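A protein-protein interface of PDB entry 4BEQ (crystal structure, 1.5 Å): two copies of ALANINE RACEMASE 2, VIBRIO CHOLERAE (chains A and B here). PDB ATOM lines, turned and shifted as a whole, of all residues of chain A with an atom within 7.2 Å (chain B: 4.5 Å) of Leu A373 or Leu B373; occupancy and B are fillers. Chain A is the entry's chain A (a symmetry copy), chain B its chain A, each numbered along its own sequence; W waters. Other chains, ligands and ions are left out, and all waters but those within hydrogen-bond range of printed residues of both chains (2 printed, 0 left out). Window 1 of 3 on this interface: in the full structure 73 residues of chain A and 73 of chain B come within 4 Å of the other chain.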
ATOM      1  N   LEU A  22     -27.034   1.884   6.705  1.00  0.00           N
ATOM      2  CA  LEU A  22     -26.733   0.620   7.355  1.00  0.00           C
ATOM      3  C   LEU A  22     -27.988   0.092   8.011  1.00  0.00           C
ATOM      4  O   LEU A  22     -28.752   0.839   8.595  1.00  0.00           O
ATOM      5  CB  LEU A  22     -25.654   0.790   8.423  1.00  0.00           C
ATOM      6  CG  LEU A  22     -24.288   1.268   7.958  1.00  0.00           C
ATOM      7  CD1 LEU A  22     -23.337   1.318   9.145  1.00  0.00           C
ATOM      8  CD2 LEU A  22     -23.743   0.324   6.900  1.00  0.00           C
ATOM      9  N   ALA A  52     -15.515   3.430  18.668  1.00  0.00           N
ATOM     10  CA  ALA A  52     -15.882   3.762  17.297  1.00  0.00           C
ATOM     11  C   ALA A  52     -17.403   3.686  17.066  1.00  0.00           C
ATOM     12  O   ALA A  52     -17.885   3.089  16.087  1.00  0.00           O
ATOM     13  CB  ALA A  52     -15.107   2.884  16.279  1.00  0.00           C
ATOM     14  N   TYR A  55     -18.532   0.151  17.043  1.00  0.00           N
ATOM     15  CA  TYR A  55     -17.979  -0.558  15.878  1.00  0.00           C
ATOM     16  C   TYR A  55     -18.799  -0.225  14.616  1.00  0.00           C
ATOM     17  O   TYR A  55     -19.045  -1.070  13.747  1.00  0.00           O
ATOM     18  CB  TYR A  55     -17.879  -2.069  16.120  1.00  0.00           C
ATOM     19  CG  TYR A  55     -16.768  -2.506  17.061  1.00  0.00           C
ATOM     20  CD1 TYR A  55     -16.647  -1.969  18.315  1.00  0.00           C
ATOM     21  CD2 TYR A  55     -15.864  -3.494  16.676  1.00  0.00           C
ATOM     22  CE1 TYR A  55     -15.626  -2.374  19.173  1.00  0.00           C
ATOM     23  CE2 TYR A  55     -14.853  -3.911  17.518  1.00  0.00           C
ATOM     24  CZ  TYR A  55     -14.738  -3.349  18.770  1.00  0.00           C
ATOM     25  OH  TYR A  55     -13.752  -3.759  19.651  1.00  0.00           O
ATOM     26  N   GLY A  56     -19.221   1.038  14.520  1.00  0.00           N
ATOM     27  CA  GLY A  56     -20.014   1.531  13.412  1.00  0.00           C
ATOM     28  C   GLY A  56     -21.498   1.269  13.523  1.00  0.00           C
ATOM     29  O   GLY A  56     -22.303   1.795  12.749  1.00  0.00           O
ATOM     30  N   GLY A 294     -21.004   5.959  -3.164  1.00  0.00           N
ATOM     31  CA  GLY A 294     -19.631   6.006  -3.638  1.00  0.00           C
ATOM     32  C   GLY A 294     -18.629   5.987  -2.520  1.00  0.00           C
ATOM     33  O   GLY A 294     -18.962   5.629  -1.382  1.00  0.00           O
ATOM     34  N   TYR A 295     -17.390   6.354  -2.800  1.00  0.00           N
ATOM     35  CA  TYR A 295     -16.369   6.181  -1.786  1.00  0.00           C
ATOM     36  C   TYR A 295     -16.535   7.149  -0.618  1.00  0.00           C
ATOM     37  O   TYR A 295     -16.049   6.865   0.458  1.00  0.00           O
ATOM     38  CB  TYR A 295     -14.935   6.199  -2.356  1.00  0.00           C
ATOM     39  CG  TYR A 295     -14.492   7.443  -3.119  1.00  0.00           C
ATOM     40  CD1 TYR A 295     -14.242   8.635  -2.473  1.00  0.00           C
ATOM     41  CD2 TYR A 295     -14.307   7.393  -4.492  1.00  0.00           C
ATOM     42  CE1 TYR A 295     -13.827   9.739  -3.164  1.00  0.00           C
ATOM     43  CE2 TYR A 295     -13.859   8.511  -5.199  1.00  0.00           C
ATOM     44  CZ  TYR A 295     -13.640   9.677  -4.529  1.00  0.00           C
ATOM     45  OH  TYR A 295     -13.227  10.810  -5.224  1.00  0.00           O
ATOM     46  N   SER A 296     -17.249   8.264  -0.814  1.00  0.00           N
ATOM     47  CA  SER A 296     -17.475   9.191   0.299  1.00  0.00           C
ATOM     48  C   SER A 296     -18.513   8.624   1.269  1.00  0.00           C
ATOM     49  O   SER A 296     -18.667   9.148   2.373  1.00  0.00           O
ATOM     50  CB  SER A 296     -17.896  10.585  -0.178  1.00  0.00           C
ATOM     51  OG  SER A 296     -19.146  10.591  -0.834  1.00  0.00           O
ATOM     52  N   ASP A 297     -19.211   7.559   0.867  1.00  0.00           N
ATOM     53  CA  ASP A 297     -20.090   6.820   1.789  1.00  0.00           C
ATOM     54  C   ASP A 297     -19.387   5.624   2.392  1.00  0.00           C
ATOM     55  O   ASP A 297     -19.987   4.888   3.193  1.00  0.00           O
ATOM     56  CB  ASP A 297     -21.313   6.327   1.024  1.00  0.00           C
ATOM     57  CG  ASP A 297     -21.995   7.434   0.268  1.00  0.00           C
ATOM     58  OD1 ASP A 297     -22.605   8.304   0.921  1.00  0.00           O
ATOM     59  OD2 ASP A 297     -21.905   7.433  -0.979  1.00  0.00           O
ATOM     60  N   GLY A 298     -18.138   5.396   1.989  1.00  0.00           N
ATOM     61  CA  GLY A 298     -17.384   4.243   2.475  1.00  0.00           C
ATOM     62  C   GLY A 298     -17.435   2.992   1.597  1.00  0.00           C
ATOM     63  O   GLY A 298     -17.060   1.893   2.059  1.00  0.00           O
ATOM     64  N   TYR A 299     -17.867   3.137   0.339  1.00  0.00           N
ATOM     65  CA  TYR A 299     -17.821   2.053  -0.630  1.00  0.00           C
ATOM     66  C   TYR A 299     -16.617   2.328  -1.523  1.00  0.00           C
ATOM     67  O   TYR A 299     -16.693   3.194  -2.380  1.00  0.00           O
ATOM     68  CB  TYR A 299     -19.121   1.993  -1.443  1.00  0.00           C
ATOM     69  CG  TYR A 299     -19.294   0.671  -2.185  1.00  0.00           C
ATOM     70  CD1 TYR A 299     -19.520  -0.507  -1.501  1.00  0.00           C
ATOM     71  CD2 TYR A 299     -19.209   0.619  -3.559  1.00  0.00           C
ATOM     72  CE1 TYR A 299     -19.662  -1.708  -2.185  1.00  0.00           C
ATOM     73  CE2 TYR A 299     -19.355  -0.574  -4.254  1.00  0.00           C
ATOM     74  CZ  TYR A 299     -19.564  -1.727  -3.557  1.00  0.00           C
ATOM     75  OH  TYR A 299     -19.692  -2.923  -4.231  1.00  0.00           O
ATOM     76  N   PRO A 300     -15.486   1.622  -1.306  1.00  0.00           N
ATOM     77  CA  PRO A 300     -14.226   2.089  -1.904  1.00  0.00           C
ATOM     78  C   PRO A 300     -14.147   2.080  -3.432  1.00  0.00           C
ATOM     79  O   PRO A 300     -14.838   1.354  -4.139  1.00  0.00           O
ATOM     80  CB  PRO A 300     -13.182   1.143  -1.308  1.00  0.00           C
ATOM     81  CG  PRO A 300     -13.807   0.625  -0.056  1.00  0.00           C
ATOM     82  CD  PRO A 300     -15.259   0.526  -0.350  1.00  0.00           C
ATOM     83  N   LEU A 365      -8.948  -4.018   2.255  1.00  0.00           N
ATOM     84  CA  LEU A 365      -8.995  -3.511   3.622  1.00  0.00           C
ATOM     85  C   LEU A 365      -9.436  -4.647   4.534  1.00  0.00           C
ATOM     86  O   LEU A 365     -10.035  -5.618   4.071  1.00  0.00           O
ATOM     87  CB  LEU A 365     -10.034  -2.397   3.777  1.00  0.00           C
ATOM     88  CG  LEU A 365      -9.815  -1.089   3.006  1.00  0.00           C
ATOM     89  CD1 LEU A 365     -11.041  -0.195   3.093  1.00  0.00           C
ATOM     90  CD2 LEU A 365      -8.600  -0.377   3.537  1.00  0.00           C
ATOM     91  N   PHE A 367     -12.110  -5.868   7.456  1.00  0.00           N
ATOM     92  CA  PHE A 367     -13.540  -5.599   7.628  1.00  0.00           C
ATOM     93  C   PHE A 367     -13.809  -4.381   8.529  1.00  0.00           C
ATOM     94  O   PHE A 367     -14.581  -3.513   8.127  1.00  0.00           O
ATOM     95  CB  PHE A 367     -14.224  -6.870   8.149  1.00  0.00           C
ATOM     96  CG  PHE A 367     -15.755  -6.828   8.201  1.00  0.00           C
ATOM     97  CD1 PHE A 367     -16.526  -6.217   7.236  1.00  0.00           C
ATOM     98  CD2 PHE A 367     -16.415  -7.493   9.235  1.00  0.00           C
ATOM     99  CE1 PHE A 367     -17.940  -6.222   7.330  1.00  0.00           C
ATOM    100  CE2 PHE A 367     -17.799  -7.504   9.314  1.00  0.00           C
ATOM    101  CZ  PHE A 367     -18.560  -6.874   8.366  1.00  0.00           C
ATOM    102  N   PRO A 368     -13.180  -4.293   9.722  1.00  0.00           N
ATOM    103  CA  PRO A 368     -13.456  -3.110  10.553  1.00  0.00           C
ATOM    104  C   PRO A 368     -13.008  -1.779   9.946  1.00  0.00           C
ATOM    105  O   PRO A 368     -13.569  -0.726  10.300  1.00  0.00           O
ATOM    106  CB  PRO A 368     -12.724  -3.404  11.864  1.00  0.00           C
ATOM    107  CG  PRO A 368     -11.734  -4.470  11.534  1.00  0.00           C
ATOM    108  CD  PRO A 368     -12.331  -5.276  10.429  1.00  0.00           C
ATOM    109  N   GLU A 369     -12.047  -1.791   9.040  1.00  0.00           N
ATOM    110  CA  GLU A 369     -11.726  -0.554   8.342  1.00  0.00           C
ATOM    111  C   GLU A 369     -12.915  -0.076   7.547  1.00  0.00           C
ATOM    112  O   GLU A 369     -13.157   1.142   7.442  1.00  0.00           O
ATOM    113  CB  GLU A 369     -10.528  -0.728   7.425  1.00  0.00           C
ATOM    114  CG  GLU A 369      -9.212  -0.778   8.178  1.00  0.00           C
ATOM    115  CD  GLU A 369      -8.042  -0.897   7.226  1.00  0.00           C
ATOM    116  OE1 GLU A 369      -7.801  -2.011   6.698  1.00  0.00           O
ATOM    117  OE2 GLU A 369      -7.386   0.131   7.000  1.00  0.00           O
ATOM    118  N   LEU A 370     -13.619  -1.007   6.927  1.00  0.00           N
ATOM    119  CA  LEU A 370     -14.844  -0.700   6.198  1.00  0.00           C
ATOM    120  C   LEU A 370     -15.960  -0.225   7.121  1.00  0.00           C
ATOM    121  O   LEU A 370     -16.526   0.866   6.925  1.00  0.00           O
ATOM    122  CB  LEU A 370     -15.311  -1.909   5.394  1.00  0.00           C
ATOM    123  CG  LEU A 370     -14.482  -2.221   4.142  1.00  0.00           C
ATOM    124  CD1 LEU A 370     -14.708  -3.633   3.654  1.00  0.00           C
ATOM    125  CD2 LEU A 370     -14.814  -1.230   3.029  1.00  0.00           C
ATOM    126  N   TYR A 371     -16.318  -1.047   8.103  1.00  0.00           N
ATOM    127  CA  TYR A 371     -17.568  -0.788   8.813  1.00  0.00           C
ATOM    128  C   TYR A 371     -17.494   0.395   9.772  1.00  0.00           C
ATOM    129  O   TYR A 371     -18.516   1.054  10.018  1.00  0.00           O
ATOM    130  CB  TYR A 371     -18.151  -2.064   9.443  1.00  0.00           C
ATOM    131  CG  TYR A 371     -17.379  -2.767  10.533  1.00  0.00           C
ATOM    132  CD1 TYR A 371     -17.083  -2.138  11.737  1.00  0.00           C
ATOM    133  CD2 TYR A 371     -16.995  -4.103  10.390  1.00  0.00           C
ATOM    134  CE1 TYR A 371     -16.416  -2.809  12.757  1.00  0.00           C
ATOM    135  CE2 TYR A 371     -16.355  -4.776  11.406  1.00  0.00           C
ATOM    136  CZ  TYR A 371     -16.053  -4.128  12.570  1.00  0.00           C
ATOM    137  OH  TYR A 371     -15.407  -4.821  13.573  1.00  0.00           O
ATOM    138  N   THR A 372     -16.311   0.719  10.283  1.00  0.00           N
ATOM    139  CA  THR A 372     -16.226   1.862  11.187  1.00  0.00           C
ATOM    140  C   THR A 372     -16.504   3.151  10.441  1.00  0.00           C
ATOM    141  O   THR A 372     -17.188   4.035  10.933  1.00  0.00           O
ATOM    142  CB  THR A 372     -14.903   1.959  11.964  1.00  0.00           C
ATOM    143  OG1 THR A 372     -13.797   1.976  11.073  1.00  0.00           O
ATOM    144  CG2 THR A 372     -14.790   0.805  12.952  1.00  0.00           C
ATOM    145  N   LEU A 373     -16.014   3.231   9.215  1.00  0.00           N
ATOM    146  CA  LEU A 373     -16.261   4.410   8.374  1.00  0.00           C
ATOM    147  C   LEU A 373     -17.644   4.350   7.715  1.00  0.00           C
ATOM    148  O   LEU A 373     -18.264   5.387   7.460  1.00  0.00           O
ATOM    149  CB  LEU A 373     -15.123   4.615   7.372  1.00  0.00           C
ATOM    150  CG  LEU A 373     -13.739   4.753   8.038  1.00  0.00           C
ATOM    151  CD1 LEU A 373     -12.635   5.026   7.008  1.00  0.00           C
ATOM    152  CD2 LEU A 373     -13.758   5.872   9.096  1.00  0.00           C
ATOM    153  N   TRP A 374     -18.190   3.164   7.476  1.00  0.00           N
ATOM    154  CA  TRP A 374     -19.607   3.118   7.097  1.00  0.00           C
ATOM    155  C   TRP A 374     -20.453   3.817   8.165  1.00  0.00           C
ATOM    156  O   TRP A 374     -21.412   4.554   7.864  1.00  0.00           O
ATOM    157  CB  TRP A 374     -20.114   1.681   7.001  1.00  0.00           C
ATOM    158  CG  TRP A 374     -19.565   0.894   5.864  1.00  0.00           C
ATOM    159  CD1 TRP A 374     -18.877   1.365   4.769  1.00  0.00           C
ATOM    160  CD2 TRP A 374     -19.657  -0.523   5.695  1.00  0.00           C
ATOM    161  NE1 TRP A 374     -18.530   0.321   3.940  1.00  0.00           N
ATOM    162  CE2 TRP A 374     -19.012  -0.850   4.483  1.00  0.00           C
ATOM    163  CE3 TRP A 374     -20.231  -1.550   6.448  1.00  0.00           C
ATOM    164  CZ2 TRP A 374     -18.916  -2.160   4.028  1.00  0.00           C
ATOM    165  CZ3 TRP A 374     -20.132  -2.852   5.991  1.00  0.00           C
ATOM    166  CH2 TRP A 374     -19.488  -3.139   4.794  1.00  0.00           C
ATOM    167  N   GLY A 375     -20.092   3.571   9.420  1.00  0.00           N
ATOM    168  CA  GLY A 375     -20.850   4.054  10.555  1.00  0.00           C
ATOM    169  C   GLY A 375     -20.782   5.549  10.787  1.00  0.00           C
ATOM    170  O   GLY A 375     -21.730   6.123  11.302  1.00  0.00           O
ATOM    171  N   THR A 376     -19.673   6.181  10.425  1.00  0.00           N
ATOM    172  CA  THR A 376     -19.584   7.625  10.546  1.00  0.00           C
ATOM    173  C   THR A 376     -20.198   8.324   9.345  1.00  0.00           C
ATOM    174  O   THR A 376     -20.424   9.550   9.398  1.00  0.00           O
ATOM    175  CB  THR A 376     -18.132   8.105  10.654  1.00  0.00           C
ATOM    176  OG1 THR A 376     -17.407   7.606   9.520  1.00  0.00           O
ATOM    177  CG2 THR A 376     -17.469   7.641  11.971  1.00  0.00           C
ATOM    178  N   SER A 377     -20.477   7.572   8.285  1.00  0.00           N
ATOM    179  CA  SER A 377     -20.804   8.175   6.975  1.00  0.00           C
ATOM    180  C   SER A 377     -22.223   7.875   6.455  1.00  0.00           C
ATOM    181  O   SER A 377     -22.601   8.289   5.362  1.00  0.00           O
ATOM    182  CB  SER A 377     -19.778   7.749   5.931  1.00  0.00           C
ATOM    183  OG  SER A 377     -18.461   7.963   6.377  1.00  0.00           O
ATOM    184  N   ASN A 378     -23.030   7.170   7.254  1.00  0.00           N
ATOM    185  CA  ASN A 378     -24.359   6.703   6.853  1.00  0.00           C
ATOM    186  C   ASN A 378     -25.244   6.550   8.066  1.00  0.00           C
ATOM    187  O   ASN A 378     -24.749   6.177   9.135  1.00  0.00           O
ATOM    188  CB  ASN A 378     -24.262   5.314   6.198  1.00  0.00           C
ATOM    189  CG  ASN A 378     -23.429   5.320   4.940  1.00  0.00           C
ATOM    190  OD1 ASN A 378     -23.899   5.716   3.862  1.00  0.00           O
ATOM    191  ND2 ASN A 378     -22.178   4.885   5.066  1.00  0.00           N
ATOM    192  N   TYR B 295      -7.772   3.896  12.494  1.00  0.00           N
ATOM    193  CA  TYR B 295      -8.447   3.784  11.216  1.00  0.00           C
ATOM    194  C   TYR B 295      -9.921   4.170  11.297  1.00  0.00           C
ATOM    195  O   TYR B 295     -10.494   4.526  10.288  1.00  0.00           O
ATOM    196  CB  TYR B 295      -8.242   2.413  10.538  1.00  0.00           C
ATOM    197  CG  TYR B 295      -8.688   1.171  11.304  1.00  0.00           C
ATOM    198  CD1 TYR B 295     -10.022   0.874  11.483  1.00  0.00           C
ATOM    199  CD2 TYR B 295      -7.748   0.292  11.820  1.00  0.00           C
ATOM    200  CE1 TYR B 295     -10.411  -0.252  12.154  1.00  0.00           C
ATOM    201  CE2 TYR B 295      -8.140  -0.872  12.485  1.00  0.00           C
ATOM    202  CZ  TYR B 295      -9.468  -1.122  12.659  1.00  0.00           C
ATOM    203  OH  TYR B 295      -9.876  -2.260  13.350  1.00  0.00           O
ATOM    204  N   SER B 296     -10.521   4.140  12.493  1.00  0.00           N
ATOM    205  CA  SER B 296     -11.920   4.556  12.619  1.00  0.00           C
ATOM    206  C   SER B 296     -12.040   6.078  12.530  1.00  0.00           C
ATOM    207  O   SER B 296     -13.148   6.596  12.387  1.00  0.00           O
ATOM    208  CB  SER B 296     -12.569   4.044  13.910  1.00  0.00           C
ATOM    209  OG  SER B 296     -11.986   4.590  15.075  1.00  0.00           O
ATOM    210  N   GLY B 298     -10.211   7.487  10.132  1.00  0.00           N
ATOM    211  CA  GLY B 298      -9.783   7.664   8.746  1.00  0.00           C
ATOM    212  C   GLY B 298      -8.273   7.710   8.513  1.00  0.00           C
ATOM    213  O   GLY B 298      -7.825   8.129   7.424  1.00  0.00           O
ATOM    214  N   GLU B 369     -10.416   9.814  -1.401  1.00  0.00           N
ATOM    215  CA  GLU B 369     -10.886   8.699  -0.589  1.00  0.00           C
ATOM    216  C   GLU B 369     -10.563   8.936   0.864  1.00  0.00           C
ATOM    217  O   GLU B 369     -11.353   8.571   1.756  1.00  0.00           O
ATOM    218  CB  GLU B 369     -10.280   7.384  -1.045  1.00  0.00           C
ATOM    219  CG  GLU B 369     -10.903   6.863  -2.327  1.00  0.00           C
ATOM    220  CD  GLU B 369     -10.310   5.526  -2.717  1.00  0.00           C
ATOM    221  OE1 GLU B 369      -9.170   5.498  -3.242  1.00  0.00           O
ATOM    222  OE2 GLU B 369     -10.985   4.513  -2.478  1.00  0.00           O
ATOM    223  N   LEU B 370      -9.384   9.475   1.123  1.00  0.00           N
ATOM    224  CA  LEU B 370      -8.975   9.843   2.474  1.00  0.00           C
ATOM    225  C   LEU B 370      -9.815  10.982   3.039  1.00  0.00           C
ATOM    226  O   LEU B 370     -10.414  10.853   4.123  1.00  0.00           O
ATOM    227  CB  LEU B 370      -7.497  10.216   2.508  1.00  0.00           C
ATOM    228  CG  LEU B 370      -6.522   9.039   2.386  1.00  0.00           C
ATOM    229  CD1 LEU B 370      -5.136   9.493   1.991  1.00  0.00           C
ATOM    230  CD2 LEU B 370      -6.458   8.269   3.703  1.00  0.00           C
ATOM    231  N   TYR B 371      -9.834  12.116   2.346  1.00  0.00           N
ATOM    232  CA  TYR B 371     -10.357  13.320   2.985  1.00  0.00           C
ATOM    233  C   TYR B 371     -11.875  13.330   3.126  1.00  0.00           C
ATOM    234  O   TYR B 371     -12.403  13.951   4.061  1.00  0.00           O
ATOM    235  CB  TYR B 371      -9.782  14.603   2.362  1.00  0.00           C
ATOM    236  CG  TYR B 371     -10.092  14.925   0.920  1.00  0.00           C
ATOM    237  CD1 TYR B 371     -11.397  15.128   0.483  1.00  0.00           C
ATOM    238  CD2 TYR B 371      -9.065  15.096  -0.012  1.00  0.00           C
ATOM    239  CE1 TYR B 371     -11.671  15.475  -0.835  1.00  0.00           C
ATOM    240  CE2 TYR B 371      -9.332  15.460  -1.312  1.00  0.00           C
ATOM    241  CZ  TYR B 371     -10.623  15.629  -1.722  1.00  0.00           C
ATOM    242  OH  TYR B 371     -10.868  15.991  -3.032  1.00  0.00           O
ATOM    243  N   THR B 372     -12.593  12.622   2.260  1.00  0.00           N
ATOM    244  CA  THR B 372     -14.046  12.608   2.398  1.00  0.00           C
ATOM    245  C   THR B 372     -14.453  11.884   3.666  1.00  0.00           C
ATOM    246  O   THR B 372     -15.350  12.306   4.378  1.00  0.00           O
ATOM    247  CB  THR B 372     -14.793  12.036   1.183  1.00  0.00           C
ATOM    248  OG1 THR B 372     -14.333  10.726   0.881  1.00  0.00           O
ATOM    249  CG2 THR B 372     -14.628  12.960  -0.016  1.00  0.00           C
ATOM    250  N   LEU B 373     -13.742  10.814   3.977  1.00  0.00           N
ATOM    251  CA  LEU B 373     -14.009  10.058   5.209  1.00  0.00           C
ATOM    252  C   LEU B 373     -13.361  10.725   6.428  1.00  0.00           C
ATOM    253  O   LEU B 373     -13.874  10.624   7.547  1.00  0.00           O
ATOM    254  CB  LEU B 373     -13.614   8.588   5.045  1.00  0.00           C
ATOM    255  CG  LEU B 373     -14.324   7.893   3.865  1.00  0.00           C
ATOM    256  CD1 LEU B 373     -13.957   6.406   3.775  1.00  0.00           C
ATOM    257  CD2 LEU B 373     -15.851   8.051   3.985  1.00  0.00           C
ATOM    258  N   TRP B 374     -12.270  11.461   6.253  1.00  0.00           N
ATOM    259  CA  TRP B 374     -11.817  12.304   7.366  1.00  0.00           C
ATOM    260  C   TRP B 374     -12.950  13.238   7.805  1.00  0.00           C
ATOM    261  O   TRP B 374     -13.173  13.478   9.006  1.00  0.00           O
ATOM    262  CB  TRP B 374     -10.645  13.191   6.956  1.00  0.00           C
ATOM    263  CG  TRP B 374      -9.368  12.471   6.702  1.00  0.00           C
ATOM    264  CD1 TRP B 374      -9.055  11.172   7.034  1.00  0.00           C
ATOM    265  CD2 TRP B 374      -8.209  13.007   6.059  1.00  0.00           C
ATOM    266  NE1 TRP B 374      -7.774  10.873   6.624  1.00  0.00           N
ATOM    267  CE2 TRP B 374      -7.229  11.992   6.033  1.00  0.00           C
ATOM    268  CE3 TRP B 374      -7.900  14.252   5.507  1.00  0.00           C
ATOM    269  CZ2 TRP B 374      -5.977  12.188   5.461  1.00  0.00           C
ATOM    270  CZ3 TRP B 374      -6.653  14.444   4.939  1.00  0.00           C
ATOM    271  CH2 TRP B 374      -5.712  13.421   4.929  1.00  0.00           C
ATOM    272  N   GLY B 375     -13.657  13.770   6.813  1.00  0.00           N
ATOM    273  CA  GLY B 375     -14.686  14.762   7.039  1.00  0.00           C
ATOM    274  C   GLY B 375     -15.942  14.248   7.711  1.00  0.00           C
ATOM    275  O   GLY B 375     -16.598  14.998   8.418  1.00  0.00           O
ATOM    276  N   THR B 376     -16.287  12.986   7.492  1.00  0.00           N
ATOM    277  CA  THR B 376     -17.434  12.415   8.176  1.00  0.00           C
ATOM    278  C   THR B 376     -17.064  11.918   9.563  1.00  0.00           C
ATOM    279  O   THR B 376     -17.969  11.626  10.371  1.00  0.00           O
ATOM    280  CB  THR B 376     -18.025  11.224   7.413  1.00  0.00           C
ATOM    281  OG1 THR B 376     -16.981  10.262   7.200  1.00  0.00           O
ATOM    282  CG2 THR B 376     -18.649  11.656   6.067  1.00  0.00           C
ATOM    283  N   SER B 377     -15.769  11.831   9.849  1.00  0.00           N
ATOM    284  CA  SER B 377     -15.289  11.101  11.043  1.00  0.00           C
ATOM    285  C   SER B 377     -14.556  11.968  12.086  1.00  0.00           C
ATOM    286  O   SER B 377     -14.078  11.472  13.103  1.00  0.00           O
ATOM    287  CB  SER B 377     -14.395   9.941  10.625  1.00  0.00           C
ATOM    288  OG  SER B 377     -15.003   9.142   9.639  1.00  0.00           O
HETATM  289  O   HOH W   1     -10.811   2.521   8.358  1.00  0.00           O
HETATM  290  O   HOH W   2     -13.248   6.819   0.496  1.00  0.00           O
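The side-chain hydroxyl (OG) of Ser B377 is in hydrogen-bond range of the side-chain hydroxyl (OG1) of Thr A376 (2.9 Å).
The side-chain hydroxyl (OG) of Ser A377 lies within hydrogen-bond range of the side-chain hydroxyl (OG1) of Thr B376 (2.9 Å).
The backbone carbonyl oxygen (O) of Thr B376 lies close to the backbone carbonyl oxygen (O) of Thr A376, at 3.4 Å.
OG1 of Thr A372 lies within hydrogen-bond range of O of Pro A368 (2.8 Å).
The backbone carbonyl oxygen (O) of Leu B373 is in hydrogen-bond range of the side-chain hydroxyl (OG1) of Thr B376 (3.1 Å).
The side-chain hydroxyl of Thr A376 lies within hydrogen-bond range of the side-chain hydroxyl of Ser A377, 3.3 Å away.
O of Leu A373 lies within hydrogen-bond range of OG1 of Thr A376.
The side-chain hydroxyl (OG1) of Thr B376 lies within hydrogen-bond range of the side-chain hydroxyl (OG) of Ser B377, at 3.3 Å.
The backbone carbonyl oxygen (O) of Leu A373 lies within hydrogen-bond range of the side-chain hydroxyl (OG) of Ser A377 (2.8 Å).
Among the printed residues, pairs that only touch across the chains: Ala A52 with Ser B296 (3.7 Å), Tyr A295 with Glu B369 (3.7 Å), Tyr A295 with Thr B372 (3.95 Å), Tyr A295 with Leu B373 (3.7 Å), Ser A296 with Thr B372 (3.5 Å), Ser A296 with Leu B373 (3.4 Å), Pro A368 with Tyr B295 (3.4 Å), Glu A369 with Tyr B295 (3.7 Å), Thr A372 with Tyr B295 (3.95 Å), Thr A372 with Ser B296 (3.5 Å), Leu A373 with Tyr B295 (3.7 Å), Leu A373 with Ser B296 (3.4 Å), Leu A373 with Leu B373 (3.8 Å), Leu A373 with Ser B377 (3.5 Å) and Ser A377 with Leu B373 (3.5 Å).
Of the printed residues of chain B, Ala A52 touches Ser B296 (3.7 Å).
Tyr A55 touches none of the printed residues of chain B.
Of the printed residues of chain B, Tyr A295 touches Glu B369, Thr B372 and Leu B373.
Printed residues of chain B within 4 Å of Pro A368: Tyr B295 (3.4 Å).
Of chain B, only Tyr B295, Ser B296, Leu B373 and Ser B377 come within 4 Å of Leu A373.
Of the printed residues of chain B, Thr A376 touches Thr B376 and Ser B377.
Printed residues of chain A within 4 Å of Ser B296: Ala A52 (3.7 Å), Thr A372 (3.5 Å) and Leu A373 (3.4 Å).
Hydrophobic or aromatic side chains of chain A within 4 Å of the printed part of chain B: Ala A52, Tyr A295, Pro A368 and Leu A373.
Among the printed residues, 18 pairs touch across the chains.
Among the printed residues, no Asp or Glu carboxylate lies within 4 Å of a Lys or Arg side-chain nitrogen of the other chain.
Tyr A295 touches Thr B372, and with the chains exchanged Thr A372 touches Tyr B295.
Ser A296 touches Thr B372, and with the chains exchanged Thr A372 touches Ser B296.
Leu A373 touches Ser B377, and with the chains exchanged Ser A377 touches Leu B373.
Thr B376 touches its own counterpart, Thr A376.
12 positions are printed for both chains.
Of the 18 pairs that touch across the chains among the printed residues, 16 have their exchanged pair printed and touching as well.
Water W1 bridges O of Tyr B295 (2.8 Å) and O of Glu A369 (2.9 Å).
Water W2 bridges the backbone carbonyl oxygen of Tyr A295 (2.8 Å) and the backbone carbonyl oxygen of Glu B369 (2.9 Å).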
